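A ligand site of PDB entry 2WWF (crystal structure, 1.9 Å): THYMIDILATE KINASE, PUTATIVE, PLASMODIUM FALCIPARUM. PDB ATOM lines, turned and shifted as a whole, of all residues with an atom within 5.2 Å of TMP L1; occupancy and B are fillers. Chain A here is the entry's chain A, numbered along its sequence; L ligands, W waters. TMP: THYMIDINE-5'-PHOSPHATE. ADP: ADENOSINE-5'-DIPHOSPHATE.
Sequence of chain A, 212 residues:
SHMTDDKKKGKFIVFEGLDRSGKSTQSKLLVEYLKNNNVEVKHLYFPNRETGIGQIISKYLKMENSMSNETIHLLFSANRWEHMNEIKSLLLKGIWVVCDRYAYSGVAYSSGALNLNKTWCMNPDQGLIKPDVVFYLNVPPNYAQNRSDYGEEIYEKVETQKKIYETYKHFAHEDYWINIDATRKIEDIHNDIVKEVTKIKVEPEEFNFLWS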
ATOM      1  N   ASP A  19      26.623  12.360  19.489  1.00  0.00           N
ATOM      2  CA  ASP A  19      26.214  11.559  18.351  1.00  0.00           C
ATOM      3  C   ASP A  19      27.054  10.253  18.215  1.00  0.00           C
ATOM      4  O   ASP A  19      28.259  10.322  18.285  1.00  0.00           O
ATOM      5  CB  ASP A  19      26.308  12.438  17.126  1.00  0.00           C
ATOM      6  CG  ASP A  19      25.214  13.522  17.167  1.00  0.00           C
ATOM      7  OD1 ASP A  19      24.074  13.212  16.731  1.00  0.00           O
ATOM      8  OD2 ASP A  19      25.465  14.568  17.817  1.00  0.00           O
ATOM      9  N   LYS A  23      23.991   5.135  22.373  1.00  0.00           N
ATOM     10  CA  LYS A  23      22.699   5.154  23.079  1.00  0.00           C
ATOM     11  C   LYS A  23      21.718   4.067  22.593  1.00  0.00           C
ATOM     12  O   LYS A  23      21.140   3.359  23.423  1.00  0.00           O
ATOM     13  CB  LYS A  23      22.036   6.604  22.978  1.00  0.00           C
ATOM     14  CG  LYS A  23      22.833   7.682  23.729  1.00  0.00           C
ATOM     15  CD  LYS A  23      22.177   9.114  23.539  1.00  0.00           C
ATOM     16  CE  LYS A  23      22.789   9.884  22.368  1.00  0.00           C
ATOM     17  NZ  LYS A  23      23.120   9.273  21.085  1.00  0.00           N
ATOM     18  N   PHE A  46      13.905  10.090  21.174  1.00  0.00           N
ATOM     19  CA  PHE A  46      13.610  11.417  20.603  1.00  0.00           C
ATOM     20  C   PHE A  46      14.800  11.836  19.731  1.00  0.00           C
ATOM     21  O   PHE A  46      15.968  11.514  20.043  1.00  0.00           O
ATOM     22  CB  PHE A  46      13.323  12.443  21.746  1.00  0.00           C
ATOM     23  CG  PHE A  46      12.021  12.150  22.458  1.00  0.00           C
ATOM     24  CD1 PHE A  46      10.798  12.479  21.843  1.00  0.00           C
ATOM     25  CD2 PHE A  46      11.993  11.522  23.690  1.00  0.00           C
ATOM     26  CE1 PHE A  46       9.579  12.155  22.468  1.00  0.00           C
ATOM     27  CE2 PHE A  46      10.773  11.243  24.313  1.00  0.00           C
ATOM     28  CZ  PHE A  46       9.587  11.549  23.730  1.00  0.00           C
ATOM     29  N   PRO A  47      14.542  12.576  18.638  1.00  0.00           N
ATOM     30  CA  PRO A  47      13.196  12.926  18.140  1.00  0.00           C
ATOM     31  C   PRO A  47      12.494  11.683  17.597  1.00  0.00           C
ATOM     32  O   PRO A  47      13.157  10.758  17.055  1.00  0.00           O
ATOM     33  CB  PRO A  47      13.492  13.898  17.013  1.00  0.00           C
ATOM     34  CG  PRO A  47      14.825  13.454  16.438  1.00  0.00           C
ATOM     35  CD  PRO A  47      15.624  13.148  17.754  1.00  0.00           C
ATOM     36  N   ARG A  49      10.816  10.675  14.631  1.00  0.00           N
ATOM     37  CA  ARG A  49      10.746  11.280  13.269  1.00  0.00           C
ATOM     38  C   ARG A  49       9.464  10.901  12.516  1.00  0.00           C
ATOM     39  O   ARG A  49       9.291  11.325  11.392  1.00  0.00           O
ATOM     40  CB  ARG A  49      12.000  10.963  12.427  1.00  0.00           C
ATOM     41  CG  ARG A  49      13.261  11.457  13.111  1.00  0.00           C
ATOM     42  CD  ARG A  49      14.469  10.877  12.408  1.00  0.00           C
ATOM     43  NE  ARG A  49      15.743  11.053  13.134  1.00  0.00           N
ATOM     44  CZ  ARG A  49      16.894  11.477  12.596  1.00  0.00           C
ATOM     45  NH1 ARG A  49      16.948  11.885  11.338  1.00  0.00           N
ATOM     46  NH2 ARG A  49      17.996  11.532  13.324  1.00  0.00           N
ATOM     47  N   LEU A  61      17.582  17.760  10.244  1.00  0.00           N
ATOM     48  CA  LEU A  61      18.795  16.979  10.610  1.00  0.00           C
ATOM     49  C   LEU A  61      19.507  16.477   9.370  1.00  0.00           C
ATOM     50  O   LEU A  61      20.725  16.409   9.351  1.00  0.00           O
ATOM     51  CB  LEU A  61      18.380  15.792  11.516  1.00  0.00           C
ATOM     52  CG  LEU A  61      17.951  16.195  12.954  1.00  0.00           C
ATOM     53  CD1 LEU A  61      17.388  14.895  13.686  1.00  0.00           C
ATOM     54  CD2 LEU A  61      19.093  16.967  13.733  1.00  0.00           C
ATOM     55  N   PHE A  76      11.579  20.496  18.612  1.00  0.00           N
ATOM     56  CA  PHE A  76      12.171  19.338  19.362  1.00  0.00           C
ATOM     57  C   PHE A  76      11.417  19.172  20.695  1.00  0.00           C
ATOM     58  O   PHE A  76      11.062  18.031  21.122  1.00  0.00           O
ATOM     59  CB  PHE A  76      13.645  19.556  19.647  1.00  0.00           C
ATOM     60  CG  PHE A  76      14.572  19.020  18.573  1.00  0.00           C
ATOM     61  CD1 PHE A  76      14.672  17.621  18.350  1.00  0.00           C
ATOM     62  CD2 PHE A  76      15.389  19.889  17.850  1.00  0.00           C
ATOM     63  CE1 PHE A  76      15.632  17.087  17.391  1.00  0.00           C
ATOM     64  CE2 PHE A  76      16.299  19.366  16.892  1.00  0.00           C
ATOM     65  CZ  PHE A  76      16.410  17.941  16.668  1.00  0.00           C
ATOM     66  N   ARG A  80       8.499  16.066  22.061  1.00  0.00           N
ATOM     67  CA  ARG A  80       8.363  15.411  23.415  1.00  0.00           C
ATOM     68  C   ARG A  80       6.972  15.529  24.018  1.00  0.00           C
ATOM     69  O   ARG A  80       6.429  14.551  24.524  1.00  0.00           O
ATOM     70  CB  ARG A  80       9.392  15.959  24.415  1.00  0.00           C
ATOM     71  CG  ARG A  80      10.846  15.469  24.077  1.00  0.00           C
ATOM     72  CD  ARG A  80      11.862  15.973  25.078  1.00  0.00           C
ATOM     73  NE  ARG A  80      12.208  17.389  24.873  1.00  0.00           N
ATOM     74  CZ  ARG A  80      13.059  17.826  23.908  1.00  0.00           C
ATOM     75  NH1 ARG A  80      13.567  16.989  23.012  1.00  0.00           N
ATOM     76  NH2 ARG A  80      13.442  19.093  23.859  1.00  0.00           N
ATOM     77  N   ARG A 101      17.489   9.709  24.409  1.00  0.00           N
ATOM     78  CA  ARG A 101      17.446  11.225  24.350  1.00  0.00           C
ATOM     79  C   ARG A 101      16.179  11.766  24.951  1.00  0.00           C
ATOM     80  O   ARG A 101      15.117  11.157  24.869  1.00  0.00           O
ATOM     81  CB  ARG A 101      17.649  11.826  22.907  1.00  0.00           C
ATOM     82  CG  ARG A 101      19.026  11.539  22.314  1.00  0.00           C
ATOM     83  CD  ARG A 101      19.203  12.388  21.002  1.00  0.00           C
ATOM     84  NE  ARG A 101      20.473  12.136  20.294  1.00  0.00           N
ATOM     85  CZ  ARG A 101      21.626  12.614  20.680  1.00  0.00           C
ATOM     86  NH1 ARG A 101      21.714  13.339  21.848  1.00  0.00           N
ATOM     87  NH2 ARG A 101      22.679  12.277  19.960  1.00  0.00           N
ATOM     88  N   TYR A 102      16.318  12.926  25.579  1.00  0.00           N
ATOM     89  CA  TYR A 102      15.202  13.641  26.104  1.00  0.00           C
ATOM     90  C   TYR A 102      15.458  15.152  26.129  1.00  0.00           C
ATOM     91  O   TYR A 102      16.164  15.701  25.249  1.00  0.00           O
ATOM     92  CB  TYR A 102      14.903  13.108  27.512  1.00  0.00           C
ATOM     93  CG  TYR A 102      13.485  13.269  28.081  1.00  0.00           C
ATOM     94  CD1 TYR A 102      12.343  12.928  27.333  1.00  0.00           C
ATOM     95  CD2 TYR A 102      13.306  13.775  29.373  1.00  0.00           C
ATOM     96  CE1 TYR A 102      11.082  13.096  27.844  1.00  0.00           C
ATOM     97  CE2 TYR A 102      11.999  13.915  29.940  1.00  0.00           C
ATOM     98  CZ  TYR A 102      10.937  13.531  29.204  1.00  0.00           C
ATOM     99  OH  TYR A 102       9.650  13.656  29.773  1.00  0.00           O
ATOM    100  N   SER A 105      19.188  16.525  25.820  1.00  0.00           N
ATOM    101  CA  SER A 105      19.632  16.744  24.423  1.00  0.00           C
ATOM    102  C   SER A 105      19.162  18.163  23.932  1.00  0.00           C
ATOM    103  O   SER A 105      19.934  18.919  23.301  1.00  0.00           O
ATOM    104  CB  SER A 105      19.030  15.693  23.479  1.00  0.00           C
ATOM    105  OG  SER A 105      19.774  14.463  23.541  1.00  0.00           O
ATOM    106  N   GLY A 106      17.881  18.446  24.135  1.00  0.00           N
ATOM    107  CA  GLY A 106      17.303  19.750  23.653  1.00  0.00           C
ATOM    108  C   GLY A 106      18.146  20.910  24.101  1.00  0.00           C
ATOM    109  O   GLY A 106      18.493  21.795  23.299  1.00  0.00           O
ATOM    110  N   TYR A 109      22.209  20.577  22.926  1.00  0.00           N
ATOM    111  CA  TYR A 109      22.449  20.778  21.476  1.00  0.00           C
ATOM    112  C   TYR A 109      22.127  22.212  21.096  1.00  0.00           C
ATOM    113  O   TYR A 109      22.898  22.846  20.397  1.00  0.00           O
ATOM    114  CB  TYR A 109      21.609  19.775  20.679  1.00  0.00           C
ATOM    115  CG  TYR A 109      22.337  18.436  20.551  1.00  0.00           C
ATOM    116  CD1 TYR A 109      23.012  18.140  19.368  1.00  0.00           C
ATOM    117  CD2 TYR A 109      22.399  17.503  21.655  1.00  0.00           C
ATOM    118  CE1 TYR A 109      23.742  16.948  19.251  1.00  0.00           C
ATOM    119  CE2 TYR A 109      23.097  16.289  21.550  1.00  0.00           C
ATOM    120  CZ  TYR A 109      23.746  16.013  20.355  1.00  0.00           C
ATOM    121  OH  TYR A 109      24.510  14.845  20.150  1.00  0.00           O
ATOM    122  N   SER A 110      20.972  22.728  21.549  1.00  0.00           N
ATOM    123  CA  SER A 110      20.578  24.115  21.187  1.00  0.00           C
ATOM    124  C   SER A 110      21.511  25.155  21.816  1.00  0.00           C
ATOM    125  O   SER A 110      21.897  26.123  21.147  1.00  0.00           O
ATOM    126  CB  SER A 110      19.118  24.410  21.551  1.00  0.00           C
ATOM    127  OG  SER A 110      18.305  23.674  20.677  1.00  0.00           O
ATOM    128  N   GLU A 153      24.449  13.581   9.422  1.00  0.00           N
ATOM    129  CA  GLU A 153      23.469  14.580   9.871  1.00  0.00           C
ATOM    130  C   GLU A 153      24.085  15.848  10.430  1.00  0.00           C
ATOM    131  O   GLU A 153      25.273  15.897  10.719  1.00  0.00           O
ATOM    132  CB  GLU A 153      22.462  13.953  10.864  1.00  0.00           C
ATOM    133  CG  GLU A 153      21.609  12.923  10.017  1.00  0.00           C
ATOM    134  CD  GLU A 153      20.427  12.310  10.783  1.00  0.00           C
ATOM    135  OE1 GLU A 153      20.302  12.503  12.000  1.00  0.00           O
ATOM    136  OE2 GLU A 153      19.595  11.668  10.141  1.00  0.00           O
ATOM    137  N   TYR A 155      24.601  17.913  13.015  1.00  0.00           N
ATOM    138  CA  TYR A 155      25.465  18.226  14.143  1.00  0.00           C
ATOM    139  C   TYR A 155      26.750  17.353  14.179  1.00  0.00           C
ATOM    140  O   TYR A 155      27.607  17.546  15.024  1.00  0.00           O
ATOM    141  CB  TYR A 155      24.689  18.113  15.478  1.00  0.00           C
ATOM    142  CG  TYR A 155      23.552  19.115  15.567  1.00  0.00           C
ATOM    143  CD1 TYR A 155      23.769  20.480  15.216  1.00  0.00           C
ATOM    144  CD2 TYR A 155      22.268  18.713  16.022  1.00  0.00           C
ATOM    145  CE1 TYR A 155      22.755  21.418  15.355  1.00  0.00           C
ATOM    146  CE2 TYR A 155      21.223  19.623  16.144  1.00  0.00           C
ATOM    147  CZ  TYR A 155      21.490  20.986  15.804  1.00  0.00           C
ATOM    148  OH  TYR A 155      20.465  21.882  15.927  1.00  0.00           O
ATOM    149  N   GLU A 156      26.898  16.448  13.216  1.00  0.00           N
ATOM    150  CA  GLU A 156      27.988  15.414  13.277  1.00  0.00           C
ATOM    151  C   GLU A 156      29.247  15.957  12.595  1.00  0.00           C
ATOM    152  O   GLU A 156      29.687  15.463  11.583  1.00  0.00           O
ATOM    153  CB  GLU A 156      27.507  14.130  12.632  1.00  0.00           C
ATOM    154  CG  GLU A 156      26.245  13.607  13.367  1.00  0.00           C
ATOM    155  CD  GLU A 156      25.784  12.227  12.904  1.00  0.00           C
ATOM    156  OE1 GLU A 156      26.078  11.836  11.761  1.00  0.00           O
ATOM    157  OE2 GLU A 156      25.075  11.533  13.697  1.00  0.00           O
HETATM  158  P   TMP L   1      19.922  10.738  16.880  1.00  0.00           P
HETATM  159  O1P TMP L   1      19.581  10.727  18.223  1.00  0.00           O
HETATM  160  O2P TMP L   1      21.311  11.150  16.891  1.00  0.00           O
HETATM  161  O3P TMP L   1      19.957   9.801  15.868  1.00  0.00           O
HETATM  162  O5' TMP L   1      19.625  12.231  16.111  1.00  0.00           O
HETATM  163  C5' TMP L   1      19.068  13.284  16.761  1.00  0.00           C
HETATM  164  C4' TMP L   1      19.849  14.551  16.459  1.00  0.00           C
HETATM  165  O4' TMP L   1      18.992  15.569  17.056  1.00  0.00           O
HETATM  166  C3' TMP L   1      21.084  14.505  17.375  1.00  0.00           C
HETATM  167  O3' TMP L   1      22.172  15.243  16.712  1.00  0.00           O
HETATM  168  C2' TMP L   1      20.680  15.238  18.682  1.00  0.00           C
HETATM  169  C1' TMP L   1      19.718  16.294  18.083  1.00  0.00           C
HETATM  170  N1  TMP L   1      18.651  16.712  19.034  1.00  0.00           N
HETATM  171  C2  TMP L   1      18.445  18.072  19.278  1.00  0.00           C
HETATM  172  O2  TMP L   1      19.130  18.958  18.740  1.00  0.00           O
HETATM  173  N3  TMP L   1      17.448  18.506  20.197  1.00  0.00           N
HETATM  174  C4  TMP L   1      16.663  17.536  20.841  1.00  0.00           C
HETATM  175  O4  TMP L   1      15.812  17.975  21.595  1.00  0.00           O
HETATM  176  C5  TMP L   1      16.862  16.181  20.602  1.00  0.00           C
HETATM  177  C5M TMP L   1      15.952  15.055  21.303  1.00  0.00           C
HETATM  178  C6  TMP L   1      17.852  15.759  19.701  1.00  0.00           C
HETATM  179  PB  ADP L   2      23.701   6.363  19.099  1.00  0.00           P
HETATM  180  O1B ADP L   2      22.435   5.667  19.303  1.00  0.00           O
HETATM  181  O2B ADP L   2      24.320   7.022  20.320  1.00  0.00           O
HETATM  182  O3B ADP L   2      23.733   7.246  17.920  1.00  0.00           O
HETATM  183  PA  ADP L   2      24.537   3.645  18.390  1.00  0.00           P
HETATM  184  O1A ADP L   2      24.182   2.786  19.530  1.00  0.00           O
HETATM  185  O2A ADP L   2      23.711   3.545  17.135  1.00  0.00           O
HETATM  186  O3A ADP L   2      24.831   5.203  18.742  1.00  0.00           O
HETATM  187  O5' ADP L   2      26.058   3.270  17.968  1.00  0.00           O
HETATM  188  C5' ADP L   2      26.774   3.899  16.868  1.00  0.00           C
HETATM  189  C4' ADP L   2      27.718   2.843  16.213  1.00  0.00           C
HETATM  190  O4' ADP L   2      28.705   2.442  17.169  1.00  0.00           O
HETATM  191  C3' ADP L   2      26.970   1.584  15.826  1.00  0.00           C
HETATM  192  O3' ADP L   2      27.544   1.099  14.631  1.00  0.00           O
HETATM  193  C2' ADP L   2      27.233   0.652  16.993  1.00  0.00           C
HETATM  194  O2' ADP L   2      27.213  -0.719  16.642  1.00  0.00           O
HETATM  195  C1' ADP L   2      28.620   1.022  17.408  1.00  0.00           C
HETATM  196  N9  ADP L   2      28.887   0.978  18.842  1.00  0.00           N
HETATM  197  C8  ADP L   2      28.074   1.364  19.877  1.00  0.00           C
HETATM  198  N7  ADP L   2      28.717   1.225  21.089  1.00  0.00           N
HETATM  199  C5  ADP L   2      29.959   0.734  20.803  1.00  0.00           C
HETATM  200  C6  ADP L   2      31.129   0.363  21.607  1.00  0.00           C
HETATM  201  N6  ADP L   2      31.053   0.581  22.942  1.00  0.00           N
HETATM  202  N1  ADP L   2      32.236  -0.084  20.938  1.00  0.00           N
HETATM  203  C2  ADP L   2      32.266  -0.214  19.599  1.00  0.00           C
HETATM  204  N3  ADP L   2      31.213   0.077  18.813  1.00  0.00           N
HETATM  205  C4  ADP L   2      30.068   0.572  19.354  1.00  0.00           C
HETATM  206  O   HOH W   1      22.391   9.565  14.198  1.00  0.00           O
HETATM  207  O   HOH W   2      18.513   8.113  14.526  1.00  0.00           O
HETATM  208  O   HOH W   3      20.686   7.320  16.753  1.00  0.00           O
HETATM  209  O   HOH W   4      17.242   9.226  19.219  1.00  0.00           O
HETATM  210  O   HOH W   5      20.422   8.680  19.971  1.00  0.00           O
HETATM  211  O   HOH W   6      21.907  12.904  14.001  1.00  0.00           O
HETATM  212  O   HOH W   7      23.233   9.790  18.124  1.00  0.00           O
HETATM  213  O   HOH W   8      22.798  15.643  13.991  1.00  0.00           O
HETATM  214  O   HOH W   9      16.740  21.176  20.708  1.00  0.00           O
HETATM  215  O   HOH W  10      19.133  21.666  18.265  1.00  0.00           O
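Residues that only touch TMP L1: Phe 76 (3.2 Å), Tyr 109 (3.3 Å), Tyr 155 (3.4 Å), Pro 47 (3.6 Å), Leu 61 (3.6 Å), Ser 105 (3.6 Å) and Phe 46 (3.7 Å). Of the 17 residues printed, 12 come within 4 Å of TMP L1.
Water W7 lies within hydrogen-bond range of O3B of ADP L2 (2.6 Å), O2P of TMP L1 (2.7 Å), NZ of Lys 23 (3.0 Å) and NH2 of Arg 101 (3.1 Å). Water W3 bridges an oxygen (O3P) of TMP L1 (2.7 Å) and an oxygen (O3B) of ADP L2 (3.3 Å). Water W10 lies within hydrogen-bond range of OH of Tyr 155, O2 of TMP L1 and OG of Ser 110. Water W9 lies within hydrogen-bond range of a nitrogen (N3) of TMP L1 (2.8 Å), the side-chain hydroxyl of Ser 110 (2.9 Å) and the backbone carbonyl oxygen of Gly 106 (3.2 Å). Water W4 bridges the backbone carbonyl oxygen (O) of Phe 46 and an oxygen (O1P) of TMP L1. Water W1 lies within hydrogen-bond range of O3P of TMP L1 (3.0 Å) and OE2 of Glu 156 (3.4 Å).
The guanidinium group (NH1) of Arg 101 is in hydrogen-bond range of the side-chain hydroxyl (OG) of Ser 105, at 2.8 Å. NH1 of Arg 80 sits at hydrogen-bond distance from O of Phe 76 (3.3 Å). OD1 of Asp 19 lies within salt-bridge range of NH2 of Arg 101, at 3.6 Å. OH of Tyr 109 lies within hydrogen-bond range of OD2 of Asp 19, 2.5 Å away. The side-chain hydroxyl of Tyr 109 sits at hydrogen-bond distance from the guanidinium group of Arg 101. NH2 of Arg 49 lies within salt-bridge range of OE1 of Glu 153 (2.8 Å). The backbone carbonyl oxygen (O) of Gly 106 lies close to the side-chain hydroxyl (OG) of Ser 110 (3.2 Å).
The side-chain carboxylate (OD1) of Asp 19 is in hydrogen-bond range of an oxygen (O3') of TMP L1 (2.8 Å). The guanidinium group (NH2) of Arg 49 is in salt-bridge range of an oxygen (O3P) of TMP L1. The side-chain amino group (NZ) of Lys 23 is in salt-bridge range of an oxygen (O2B) of ADP L2, at 2.7 Å. The backbone NH (N) of Lys 23 is in hydrogen-bond range of an oxygen (O2B) of ADP L2, 2.8 Å away. The backbone NH of Gly 106 lies close to an oxygen (O4) of TMP L1 (3.3 Å). NE of Arg 101 lies within salt-bridge range of O1P of TMP L1 (2.7 Å). The guanidinium group (NH1) of Arg 80 sits at hydrogen-bond distance from an oxygen (O4) of TMP L1, 2.8 Å away.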
